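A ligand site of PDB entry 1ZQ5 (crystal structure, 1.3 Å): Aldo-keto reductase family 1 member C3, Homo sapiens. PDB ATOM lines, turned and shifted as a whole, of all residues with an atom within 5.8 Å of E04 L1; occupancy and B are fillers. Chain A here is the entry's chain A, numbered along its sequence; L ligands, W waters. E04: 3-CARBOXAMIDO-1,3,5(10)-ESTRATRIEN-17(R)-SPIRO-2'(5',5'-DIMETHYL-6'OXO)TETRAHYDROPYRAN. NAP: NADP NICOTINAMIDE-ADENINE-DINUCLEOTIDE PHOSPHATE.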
ATOM      1  N   TYR A  24     -20.943 -18.234  -1.469  1.00  0.00           N
ATOM      2  CA  TYR A  24     -22.207 -17.896  -2.140  1.00  0.00           C
ATOM      3  C   TYR A  24     -23.316 -17.646  -1.137  1.00  0.00           C
ATOM      4  O   TYR A  24     -23.533 -18.430  -0.217  1.00  0.00           O
ATOM      5  CB  TYR A  24     -22.667 -18.957  -3.151  1.00  0.00           C
ATOM      6  CG  TYR A  24     -23.952 -18.547  -3.844  1.00  0.00           C
ATOM      7  CD1 TYR A  24     -23.930 -17.602  -4.858  1.00  0.00           C
ATOM      8  CD2 TYR A  24     -25.192 -19.068  -3.449  1.00  0.00           C
ATOM      9  CE1 TYR A  24     -25.105 -17.195  -5.485  1.00  0.00           C
ATOM     10  CE2 TYR A  24     -26.371 -18.649  -4.050  1.00  0.00           C
ATOM     11  CZ  TYR A  24     -26.317 -17.730  -5.077  1.00  0.00           C
ATOM     12  OH  TYR A  24     -27.485 -17.328  -5.692  1.00  0.00           O
ATOM     13  N   PRO A  27     -29.179 -13.639  -3.877  1.00  0.00           N
ATOM     14  CA  PRO A  27     -29.267 -12.196  -4.142  1.00  0.00           C
ATOM     15  C   PRO A  27     -29.969 -11.376  -3.073  1.00  0.00           C
ATOM     16  O   PRO A  27     -29.721 -10.175  -2.959  1.00  0.00           O
ATOM     17  CB  PRO A  27     -30.080 -12.125  -5.436  1.00  0.00           C
ATOM     18  CG  PRO A  27     -29.848 -13.416  -6.105  1.00  0.00           C
ATOM     19  CD  PRO A  27     -29.731 -14.428  -4.996  1.00  0.00           C
ATOM     20  N   LEU A  54     -20.240 -15.570 -10.820  1.00  0.00           N
ATOM     21  CA  LEU A  54     -21.680 -15.732 -10.623  1.00  0.00           C
ATOM     22  C   LEU A  54     -22.178 -15.168  -9.285  1.00  0.00           C
ATOM     23  O   LEU A  54     -23.346 -14.778  -9.178  1.00  0.00           O
ATOM     24  CB  LEU A  54     -22.019 -17.223 -10.698  1.00  0.00           C
ATOM     25  CG  LEU A  54     -23.496 -17.627 -10.508  1.00  0.00           C
ATOM     26  CD1 LEU A  54     -24.357 -17.138 -11.664  1.00  0.00           C
ATOM     27  CD2 LEU A  54     -23.607 -19.139 -10.345  1.00  0.00           C
ATOM     28  N   TRP A  86     -17.703 -17.897 -15.596  1.00  0.00           N
ATOM     29  CA  TRP A  86     -19.129 -18.133 -15.758  1.00  0.00           C
ATOM     30  C   TRP A  86     -19.446 -18.621 -17.185  1.00  0.00           C
ATOM     31  O   TRP A  86     -18.673 -18.404 -18.128  1.00  0.00           O
ATOM     32  CB  TRP A  86     -19.968 -16.913 -15.304  1.00  0.00           C
ATOM     33  CG  TRP A  86     -21.435 -17.185 -15.424  1.00  0.00           C
ATOM     34  CD1 TRP A  86     -22.353 -16.475 -16.156  1.00  0.00           C
ATOM     35  CD2 TRP A  86     -22.131 -18.316 -14.897  1.00  0.00           C
ATOM     36  NE1 TRP A  86     -23.587 -17.073 -16.079  1.00  0.00           N
ATOM     37  CE2 TRP A  86     -23.481 -18.214 -15.323  1.00  0.00           C
ATOM     38  CE3 TRP A  86     -21.755 -19.409 -14.096  1.00  0.00           C
ATOM     39  CZ2 TRP A  86     -24.446 -19.163 -14.975  1.00  0.00           C
ATOM     40  CZ3 TRP A  86     -22.718 -20.356 -13.758  1.00  0.00           C
ATOM     41  CH2 TRP A  86     -24.041 -20.226 -14.201  1.00  0.00           C
ATOM     42  N   HIS A 117     -16.834 -22.950 -14.295  1.00  0.00           N
ATOM     43  CA  HIS A 117     -17.874 -23.120 -13.275  1.00  0.00           C
ATOM     44  C   HIS A 117     -18.800 -24.314 -13.580  1.00  0.00           C
ATOM     45  O   HIS A 117     -19.217 -25.044 -12.664  1.00  0.00           O
ATOM     46  CB  HIS A 117     -18.702 -21.831 -13.162  1.00  0.00           C
ATOM     47  CG  HIS A 117     -19.435 -21.655 -11.864  1.00  0.00           C
ATOM     48  ND1 HIS A 117     -19.549 -20.421 -11.244  1.00  0.00           N
ATOM     49  CD2 HIS A 117     -20.085 -22.533 -11.063  1.00  0.00           C
ATOM     50  CE1 HIS A 117     -20.246 -20.550 -10.132  1.00  0.00           C
ATOM     51  NE2 HIS A 117     -20.592 -21.822  -9.989  1.00  0.00           N
ATOM     52  N   SER A 118     -19.115 -24.506 -14.857  1.00  0.00           N
ATOM     53  CA  SER A 118     -20.068 -25.524 -15.269  1.00  0.00           C
ATOM     54  C   SER A 118     -19.813 -25.860 -16.742  1.00  0.00           C
ATOM     55  O   SER A 118     -19.406 -24.985 -17.501  1.00  0.00           O
ATOM     56  CB  SER A 118     -21.498 -25.024 -15.084  1.00  0.00           C
ATOM     57  OG  SER A 118     -22.452 -25.921 -15.659  1.00  0.00           O
ATOM     58  N   PRO A 119     -20.040 -27.127 -17.146  1.00  0.00           N
ATOM     59  CA  PRO A 119     -19.923 -27.441 -18.588  1.00  0.00           C
ATOM     60  C   PRO A 119     -21.076 -26.903 -19.433  1.00  0.00           C
ATOM     61  O   PRO A 119     -21.024 -26.984 -20.665  1.00  0.00           O
ATOM     62  CB  PRO A 119     -19.929 -28.975 -18.604  1.00  0.00           C
ATOM     63  CG  PRO A 119     -20.725 -29.351 -17.396  1.00  0.00           C
ATOM     64  CD  PRO A 119     -20.376 -28.315 -16.342  1.00  0.00           C
ATOM     65  N   MET A 120     -22.102 -26.345 -18.790  1.00  0.00           N
ATOM     66  CA  MET A 120     -23.322 -25.939 -19.503  1.00  0.00           C
ATOM     67  C   MET A 120     -23.194 -24.536 -20.103  1.00  0.00           C
ATOM     68  O   MET A 120     -23.696 -23.560 -19.530  1.00  0.00           O
ATOM     69  CB  MET A 120     -24.532 -26.003 -18.569  1.00  0.00           C
ATOM     70  CG  MET A 120     -24.836 -27.405 -18.062  1.00  0.00           C
ATOM     71  SD  MET A 120     -26.398 -27.451 -17.146  1.00  0.00           S
ATOM     72  CE  MET A 120     -26.074 -26.246 -15.853  1.00  0.00           C
ATOM     73  N   LEU A 128     -26.472 -12.992 -16.786  1.00  0.00           N
ATOM     74  CA  LEU A 128     -26.029 -14.210 -16.112  1.00  0.00           C
ATOM     75  C   LEU A 128     -26.798 -15.418 -16.649  1.00  0.00           C
ATOM     76  O   LEU A 128     -26.207 -16.451 -16.972  1.00  0.00           O
ATOM     77  CB  LEU A 128     -26.197 -14.103 -14.593  1.00  0.00           C
ATOM     78  CG  LEU A 128     -25.241 -13.193 -13.818  1.00  0.00           C
ATOM     79  CD1 LEU A 128     -25.664 -13.106 -12.363  1.00  0.00           C
ATOM     80  CD2 LEU A 128     -23.796 -13.662 -13.913  1.00  0.00           C
ATOM     81  N   SER A 129     -28.124 -15.250 -16.753  1.00  0.00           N
ATOM     82  CA  SER A 129     -29.014 -16.279 -17.285  1.00  0.00           C
ATOM     83  C   SER A 129     -29.768 -15.748 -18.500  1.00  0.00           C
ATOM     84  O   SER A 129     -30.895 -15.264 -18.361  1.00  0.00           O
ATOM     85  CB  SER A 129     -30.030 -16.718 -16.225  1.00  0.00           C
ATOM     86  OG  SER A 129     -29.425 -16.945 -14.968  1.00  0.00           O
ATOM     87  N   SER A 166     -15.351 -27.610 -12.848  1.00  0.00           N
ATOM     88  CA  SER A 166     -16.415 -27.787 -11.868  1.00  0.00           C
ATOM     89  C   SER A 166     -17.630 -28.332 -12.593  1.00  0.00           C
ATOM     90  O   SER A 166     -17.929 -27.945 -13.736  1.00  0.00           O
ATOM     91  CB  SER A 166     -16.714 -26.467 -11.161  1.00  0.00           C
ATOM     92  OG  SER A 166     -17.734 -26.593 -10.175  1.00  0.00           O
ATOM     93  N   ASN A 167     -18.309 -29.259 -11.924  1.00  0.00           N
ATOM     94  CA  ASN A 167     -19.552 -29.872 -12.429  1.00  0.00           C
ATOM     95  C   ASN A 167     -19.360 -30.717 -13.664  1.00  0.00           C
ATOM     96  O   ASN A 167     -20.319 -30.966 -14.389  1.00  0.00           O
ATOM     97  CB  ASN A 167     -20.635 -28.810 -12.661  1.00  0.00           C
ATOM     98  CG  ASN A 167     -21.087 -28.174 -11.375  1.00  0.00           C
ATOM     99  OD1 ASN A 167     -21.550 -28.859 -10.463  1.00  0.00           O
ATOM    100  ND2 ASN A 167     -20.957 -26.847 -11.285  1.00  0.00           N
ATOM    101  N   TYR A 216     -18.897 -29.552  -3.060  1.00  0.00           N
ATOM    102  CA  TYR A 216     -19.822 -28.492  -2.693  1.00  0.00           C
ATOM    103  C   TYR A 216     -21.182 -29.062  -2.276  1.00  0.00           C
ATOM    104  O   TYR A 216     -21.486 -30.240  -2.514  1.00  0.00           O
ATOM    105  CB  TYR A 216     -19.951 -27.426  -3.774  1.00  0.00           C
ATOM    106  CG  TYR A 216     -20.777 -27.763  -4.999  1.00  0.00           C
ATOM    107  CD1 TYR A 216     -22.171 -27.921  -4.932  1.00  0.00           C
ATOM    108  CD2 TYR A 216     -20.180 -27.848  -6.252  1.00  0.00           C
ATOM    109  CE1 TYR A 216     -22.929 -28.185  -6.062  1.00  0.00           C
ATOM    110  CE2 TYR A 216     -20.925 -28.128  -7.396  1.00  0.00           C
ATOM    111  CZ  TYR A 216     -22.306 -28.289  -7.294  1.00  0.00           C
ATOM    112  OH  TYR A 216     -23.067 -28.559  -8.406  1.00  0.00           O
ATOM    113  N   ARG A 226     -35.299 -21.784  -6.153  1.00  0.00           N
ATOM    114  CA  ARG A 226     -35.097 -21.650  -7.601  1.00  0.00           C
ATOM    115  C   ARG A 226     -34.591 -22.952  -8.212  1.00  0.00           C
ATOM    116  O   ARG A 226     -34.878 -23.272  -9.366  1.00  0.00           O
ATOM    117  CB  ARG A 226     -34.077 -20.543  -7.912  1.00  0.00           C
ATOM    118  CG  ARG A 226     -34.529 -19.138  -7.534  1.00  0.00           C
ATOM    119  CD  ARG A 226     -33.402 -18.120  -7.746  1.00  0.00           C
ATOM    120  NE  ARG A 226     -32.178 -18.501  -7.045  1.00  0.00           N
ATOM    121  CZ  ARG A 226     -31.011 -17.857  -7.131  1.00  0.00           C
ATOM    122  NH1 ARG A 226     -30.874 -16.767  -7.895  1.00  0.00           N
ATOM    123  NH2 ARG A 226     -29.974 -18.316  -6.446  1.00  0.00           N
ATOM    124  N   TRP A 227     -33.832 -23.725  -7.418  1.00  0.00           N
ATOM    125  CA  TRP A 227     -33.097 -24.876  -7.947  1.00  0.00           C
ATOM    126  C   TRP A 227     -33.353 -26.191  -7.235  1.00  0.00           C
ATOM    127  O   TRP A 227     -33.024 -27.247  -7.788  1.00  0.00           O
ATOM    128  CB  TRP A 227     -31.578 -24.607  -7.936  1.00  0.00           C
ATOM    129  CG  TRP A 227     -31.195 -23.174  -8.208  1.00  0.00           C
ATOM    130  CD1 TRP A 227     -30.629 -22.297  -7.336  1.00  0.00           C
ATOM    131  CD2 TRP A 227     -31.361 -22.466  -9.446  1.00  0.00           C
ATOM    132  NE1 TRP A 227     -30.431 -21.073  -7.941  1.00  0.00           N
ATOM    133  CE2 TRP A 227     -30.867 -21.151  -9.237  1.00  0.00           C
ATOM    134  CE3 TRP A 227     -31.884 -22.803 -10.702  1.00  0.00           C
ATOM    135  CZ2 TRP A 227     -30.885 -20.178 -10.240  1.00  0.00           C
ATOM    136  CZ3 TRP A 227     -31.893 -21.830 -11.703  1.00  0.00           C
ATOM    137  CH2 TRP A 227     -31.395 -20.526 -11.464  1.00  0.00           C
ATOM    138  N   PHE A 306     -29.404 -29.697  -6.630  1.00  0.00           N
ATOM    139  CA  PHE A 306     -29.616 -28.812  -7.772  1.00  0.00           C
ATOM    140  C   PHE A 306     -30.261 -29.646  -8.852  1.00  0.00           C
ATOM    141  O   PHE A 306     -29.646 -30.553  -9.407  1.00  0.00           O
ATOM    142  CB  PHE A 306     -28.293 -28.181  -8.240  1.00  0.00           C
ATOM    143  CG  PHE A 306     -27.765 -27.132  -7.315  1.00  0.00           C
ATOM    144  CD1 PHE A 306     -28.140 -25.802  -7.467  1.00  0.00           C
ATOM    145  CD2 PHE A 306     -26.903 -27.475  -6.269  1.00  0.00           C
ATOM    146  CE1 PHE A 306     -27.659 -24.822  -6.588  1.00  0.00           C
ATOM    147  CE2 PHE A 306     -26.410 -26.520  -5.408  1.00  0.00           C
ATOM    148  CZ  PHE A 306     -26.794 -25.190  -5.562  1.00  0.00           C
ATOM    149  N   PHE A 311     -32.070 -26.178 -16.359  1.00  0.00           N
ATOM    150  CA  PHE A 311     -30.835 -26.761 -16.878  1.00  0.00           C
ATOM    151  C   PHE A 311     -30.807 -28.283 -17.164  1.00  0.00           C
ATOM    152  O   PHE A 311     -29.877 -28.766 -17.813  1.00  0.00           O
ATOM    153  CB  PHE A 311     -29.635 -26.329 -16.013  1.00  0.00           C
ATOM    154  CG  PHE A 311     -29.811 -26.579 -14.536  1.00  0.00           C
ATOM    155  CD1 PHE A 311     -29.771 -27.886 -14.027  1.00  0.00           C
ATOM    156  CD2 PHE A 311     -29.969 -25.524 -13.653  1.00  0.00           C
ATOM    157  CE1 PHE A 311     -29.926 -28.123 -12.649  1.00  0.00           C
ATOM    158  CE2 PHE A 311     -30.116 -25.746 -12.257  1.00  0.00           C
ATOM    159  CZ  PHE A 311     -30.092 -27.045 -11.771  1.00  0.00           C
ATOM    160  N   TYR A 317     -25.630 -30.864 -19.817  1.00  0.00           N
ATOM    161  CA  TYR A 317     -26.006 -31.212 -18.452  1.00  0.00           C
ATOM    162  C   TYR A 317     -25.278 -32.511 -18.059  1.00  0.00           C
ATOM    163  O   TYR A 317     -25.352 -33.498 -18.774  1.00  0.00           O
ATOM    164  CB  TYR A 317     -27.511 -31.407 -18.401  1.00  0.00           C
ATOM    165  CG  TYR A 317     -28.106 -31.878 -17.106  1.00  0.00           C
ATOM    166  CD1 TYR A 317     -28.134 -31.057 -15.985  1.00  0.00           C
ATOM    167  CD2 TYR A 317     -28.724 -33.126 -17.026  1.00  0.00           C
ATOM    168  CE1 TYR A 317     -28.734 -31.476 -14.804  1.00  0.00           C
ATOM    169  CE2 TYR A 317     -29.323 -33.555 -15.848  1.00  0.00           C
ATOM    170  CZ  TYR A 317     -29.328 -32.729 -14.742  1.00  0.00           C
ATOM    171  OH  TYR A 317     -29.933 -33.132 -13.577  1.00  0.00           O
ATOM    172  N   PRO A 318     -24.524 -32.494 -16.952  1.00  0.00           N
ATOM    173  CA  PRO A 318     -23.646 -33.627 -16.640  1.00  0.00           C
ATOM    174  C   PRO A 318     -24.277 -34.857 -16.014  1.00  0.00           C
ATOM    175  O   PRO A 318     -23.653 -35.917 -15.993  1.00  0.00           O
ATOM    176  CB  PRO A 318     -22.638 -33.011 -15.665  1.00  0.00           C
ATOM    177  CG  PRO A 318     -23.415 -31.953 -14.962  1.00  0.00           C
ATOM    178  CD  PRO A 318     -24.343 -31.368 -16.001  1.00  0.00           C
ATOM    179  N   TYR A 319     -25.504 -34.741 -15.497  1.00  0.00           N
ATOM    180  CA  TYR A 319     -26.100 -35.867 -14.805  1.00  0.00           C
ATOM    181  C   TYR A 319     -26.850 -36.748 -15.785  1.00  0.00           C
ATOM    182  O   TYR A 319     -27.444 -36.257 -16.740  1.00  0.00           O
ATOM    183  CB  TYR A 319     -27.006 -35.412 -13.663  1.00  0.00           C
ATOM    184  CG  TYR A 319     -26.298 -34.585 -12.593  1.00  0.00           C
ATOM    185  CD1 TYR A 319     -25.017 -34.902 -12.160  1.00  0.00           C
ATOM    186  CD2 TYR A 319     -26.939 -33.490 -11.998  1.00  0.00           C
ATOM    187  CE1 TYR A 319     -24.375 -34.144 -11.195  1.00  0.00           C
ATOM    188  CE2 TYR A 319     -26.303 -32.742 -11.005  1.00  0.00           C
ATOM    189  CZ  TYR A 319     -25.025 -33.067 -10.608  1.00  0.00           C
ATOM    190  OH  TYR A 319     -24.368 -32.335  -9.627  1.00  0.00           O
HETATM  191  O26 E04 L   1     -23.468 -27.689 -13.792  1.00  0.00           O
HETATM  192  C20 E04 L   1     -24.290 -27.480 -12.913  1.00  0.00           C
HETATM  193  C21 E04 L   1     -25.254 -28.553 -12.458  1.00  0.00           C
HETATM  194  C25 E04 L   1     -24.450 -29.757 -12.003  1.00  0.00           C
HETATM  195  C24 E04 L   1     -26.147 -28.952 -13.623  1.00  0.00           C
HETATM  196  C22 E04 L   1     -26.151 -28.070 -11.303  1.00  0.00           C
HETATM  197  C23 E04 L   1     -26.515 -26.601 -11.403  1.00  0.00           C
HETATM  198  C17 E04 L   1     -25.258 -25.723 -11.342  1.00  0.00           C
HETATM  199  O19 E04 L   1     -24.314 -26.162 -12.352  1.00  0.00           O
HETATM  200  C13 E04 L   1     -25.509 -24.241 -11.597  1.00  0.00           C
HETATM  201  C18 E04 L   1     -24.173 -23.572 -11.962  1.00  0.00           C
HETATM  202  C14 E04 L   1     -26.041 -23.792 -10.232  1.00  0.00           C
HETATM  203  C15 E04 L   1     -25.053 -24.421  -9.250  1.00  0.00           C
HETATM  204  C16 E04 L   1     -24.637 -25.740  -9.930  1.00  0.00           C
HETATM  205  C8  E04 L   1     -26.363 -22.294 -10.172  1.00  0.00           C
HETATM  206  C9  E04 L   1     -27.315 -21.914 -11.322  1.00  0.00           C
HETATM  207  C11 E04 L   1     -26.846 -22.412 -12.696  1.00  0.00           C
HETATM  208  C12 E04 L   1     -26.538 -23.914 -12.685  1.00  0.00           C
HETATM  209  C10 E04 L   1     -27.619 -20.451 -11.313  1.00  0.00           C
HETATM  210  C1  E04 L   1     -28.034 -19.823 -12.505  1.00  0.00           C
HETATM  211  C2  E04 L   1     -28.344 -18.464 -12.502  1.00  0.00           C
HETATM  212  C3  E04 L   1     -28.256 -17.725 -11.330  1.00  0.00           C
HETATM  213  C27 E04 L   1     -28.586 -16.261 -11.294  1.00  0.00           C
HETATM  214  O29 E04 L   1     -28.530 -15.602 -10.136  1.00  0.00           O
HETATM  215  N28 E04 L   1     -28.935 -15.648 -12.358  1.00  0.00           N
HETATM  216  C4  E04 L   1     -27.848 -18.358 -10.153  1.00  0.00           C
HETATM  217  C5  E04 L   1     -27.542 -19.714 -10.134  1.00  0.00           C
HETATM  218  C6  E04 L   1     -27.112 -20.328  -8.803  1.00  0.00           C
HETATM  219  C7  E04 L   1     -27.035 -21.853  -8.874  1.00  0.00           C
HETATM  220  PA  NAP L   2     -23.335 -25.875   2.111  1.00  0.00           P
HETATM  221  O1A NAP L   2     -21.880 -25.782   2.435  1.00  0.00           O
HETATM  222  O2A NAP L   2     -23.880 -27.190   1.695  1.00  0.00           O
HETATM  223  O5B NAP L   2     -24.109 -25.331   3.390  1.00  0.00           O
HETATM  224  C5B NAP L   2     -25.531 -25.350   3.393  1.00  0.00           C
HETATM  225  C4B NAP L   2     -26.047 -24.620   4.623  1.00  0.00           C
HETATM  226  O4B NAP L   2     -25.512 -25.226   5.784  1.00  0.00           O
HETATM  227  C3B NAP L   2     -25.594 -23.164   4.677  1.00  0.00           C
HETATM  228  O3B NAP L   2     -26.532 -22.292   4.053  1.00  0.00           O
HETATM  229  C2B NAP L   2     -25.408 -22.900   6.168  1.00  0.00           C
HETATM  230  O2B NAP L   2     -26.370 -21.993   6.668  1.00  0.00           O
HETATM  231  C1B NAP L   2     -25.566 -24.271   6.828  1.00  0.00           C
HETATM  232  N9A NAP L   2     -24.500 -24.594   7.785  1.00  0.00           N
HETATM  233  C8A NAP L   2     -23.158 -24.319   7.660  1.00  0.00           C
HETATM  234  N7A NAP L   2     -22.528 -24.813   8.742  1.00  0.00           N
HETATM  235  C5A NAP L   2     -23.445 -25.388   9.558  1.00  0.00           C
HETATM  236  C6A NAP L   2     -23.344 -26.037  10.781  1.00  0.00           C
HETATM  237  N6A NAP L   2     -22.153 -26.215  11.362  1.00  0.00           N
HETATM  238  N1A NAP L   2     -24.495 -26.517  11.363  1.00  0.00           N
HETATM  239  C2A NAP L   2     -25.723 -26.380  10.748  1.00  0.00           C
HETATM  240  N3A NAP L   2     -25.816 -25.745   9.533  1.00  0.00           N
HETATM  241  C4A NAP L   2     -24.687 -25.266   8.957  1.00  0.00           C
HETATM  242  O3  NAP L   2     -23.705 -24.718   1.041  1.00  0.00           O
HETATM  243  PN  NAP L   2     -23.494 -24.574  -0.553  1.00  0.00           P
HETATM  244  O1N NAP L   2     -23.578 -23.134  -0.839  1.00  0.00           O
HETATM  245  O2N NAP L   2     -24.383 -25.484  -1.302  1.00  0.00           O
HETATM  246  O5D NAP L   2     -21.996 -25.086  -0.825  1.00  0.00           O
HETATM  247  C5D NAP L   2     -20.875 -24.432  -0.256  1.00  0.00           C
HETATM  248  C4D NAP L   2     -20.114 -23.584  -1.270  1.00  0.00           C
HETATM  249  O4D NAP L   2     -19.699 -24.381  -2.373  1.00  0.00           O
HETATM  250  C3D NAP L   2     -20.852 -22.397  -1.912  1.00  0.00           C
HETATM  251  O3D NAP L   2     -21.003 -21.285  -1.040  1.00  0.00           O
HETATM  252  C2D NAP L   2     -19.929 -22.152  -3.084  1.00  0.00           C
HETATM  253  O2D NAP L   2     -18.749 -21.524  -2.619  1.00  0.00           O
HETATM  254  C1D NAP L   2     -19.608 -23.594  -3.537  1.00  0.00           C
HETATM  255  N1N NAP L   2     -20.581 -24.085  -4.535  1.00  0.00           N
HETATM  256  C2N NAP L   2     -20.181 -24.207  -5.834  1.00  0.00           C
HETATM  257  C3N NAP L   2     -21.055 -24.664  -6.810  1.00  0.00           C
HETATM  258  C7N NAP L   2     -20.518 -24.910  -8.177  1.00  0.00           C
HETATM  259  O7N NAP L   2     -21.438 -25.001  -9.195  1.00  0.00           O
HETATM  260  N7N NAP L   2     -19.211 -25.052  -8.382  1.00  0.00           N
HETATM  261  C4N NAP L   2     -22.367 -24.987  -6.490  1.00  0.00           C
HETATM  262  C5N NAP L   2     -22.783 -24.865  -5.161  1.00  0.00           C
HETATM  263  C6N NAP L   2     -21.868 -24.426  -4.195  1.00  0.00           C
HETATM  264  P2B NAP L   2     -25.877 -20.672   7.454  1.00  0.00           P
HETATM  265  O1X NAP L   2     -25.208 -19.748   6.468  1.00  0.00           O
HETATM  266  O2X NAP L   2     -27.137 -20.041   8.017  1.00  0.00           O
HETATM  267  O3X NAP L   2     -24.937 -21.113   8.537  1.00  0.00           O
HETATM  268  O   HOH W   1     -29.000 -12.803  -9.884  1.00  0.00           O
HETATM  269  O   HOH W   2     -28.148 -19.664 -15.868  1.00  0.00           O
HETATM  270  O   HOH W   3     -31.696 -17.285 -13.316  1.00  0.00           O
HETATM  271  O   HOH W   4     -27.427 -15.693  -7.776  1.00  0.00           O
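The side-chain hydroxyl (OG) of Ser 118 sits at hydrogen-bond distance from an oxygen (O26) of E04 L1, at 2.8 Å. A nitrogen (N28) of E04 L1 is in hydrogen-bond range of the side-chain hydroxyl (OG) of Ser 129, 3.0 Å away. NH1 of Arg 226 lies within hydrogen-bond range of O29 of E04 L1. The side-chain amide nitrogen of Asn 167 is in hydrogen-bond range of an oxygen (O7N) of NAP L2, at 2.8 Å. An oxygen (O7N) of NAP L2 sits close to a ring nitrogen (NE2) of His 117, at 3.4 Å. N of Tyr 24 sits at hydrogen-bond distance from O3D of NAP L2 (3.1 Å). A nitrogen (N7N) of NAP L2 is in hydrogen-bond range of the side-chain hydroxyl of Ser 166 (2.8 Å).
N of Met 120 lies close to OG of Ser 118 (3.2 Å). OD1 of Asn 167 lies within hydrogen-bond range of OH of Tyr 216, at 2.6 Å. The backbone carbonyl oxygen of His 117 is in hydrogen-bond range of the side-chain amide nitrogen of Asn 167, 2.9 Å away. The side-chain hydroxyl (OG) of Ser 166 sits at hydrogen-bond distance from the side-chain amide nitrogen (ND2) of Asn 167, at 3.4 Å. NH2 of Arg 226 lies within hydrogen-bond range of OH of Tyr 24 (2.8 Å). The backbone carbonyl oxygen (O) of Leu 128 lies within hydrogen-bond range of the indole nitrogen (NE1) of Trp 86.
Leu 54 touches E04 L1 (CD1 to C3, 3.96 Å). Trp 86 touches E04 L1. Met 120 touches E04 L1 (CE to C24, 3.5 Å). Leu 128 touches E04 L1. Asn 167 touches E04 L1 (CB to O26, 3.2 Å). OH of Tyr 216 touches C16 of E04 L1, 3.6 Å away. Trp 227 touches E04 L1 (CZ2 to C5, 3.4 Å). Phe 306 touches E04 L1 (CB to C22, 3.7 Å). Phe 311 touches E04 L1 (CZ to C23, 3.6 Å). CD1 of Tyr 317 touches C24 of E04 L1, 3.7 Å away. CG of Pro 318 touches C25 of E04 L1, 3.8 Å away. OH of Tyr 319 touches C25 of E04 L1, 3.5 Å away. Hydrophobic or aromatic side chains within 4 Å of E04 L1: Leu 54, Trp 86, Met 120, Leu 128, Trp 227, Phe 306, Phe 311, Tyr 317, Pro 318 and Tyr 319. 15 residues have an atom within 4 Å of E04 L1: Leu 54, Trp 86, Ser 118, Met 120, Leu 128, Ser 129, Asn 167, Tyr 216, Arg 226, Trp 227, Phe 306, Phe 311, Tyr 317, Pro 318 and Tyr 319. The nearest printed residue that does not touch E04 L1 is Pro 119 (4.1 Å).
Water W4 bridges an oxygen (O29) of E04 L1 (2.6 Å) and the side-chain hydroxyl of Tyr 24 (2.6 Å). Water W3 bridges the side-chain hydroxyl (OG) of Ser 129 (2.8 Å) and a nitrogen (N28) of E04 L1 (3.3 Å).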
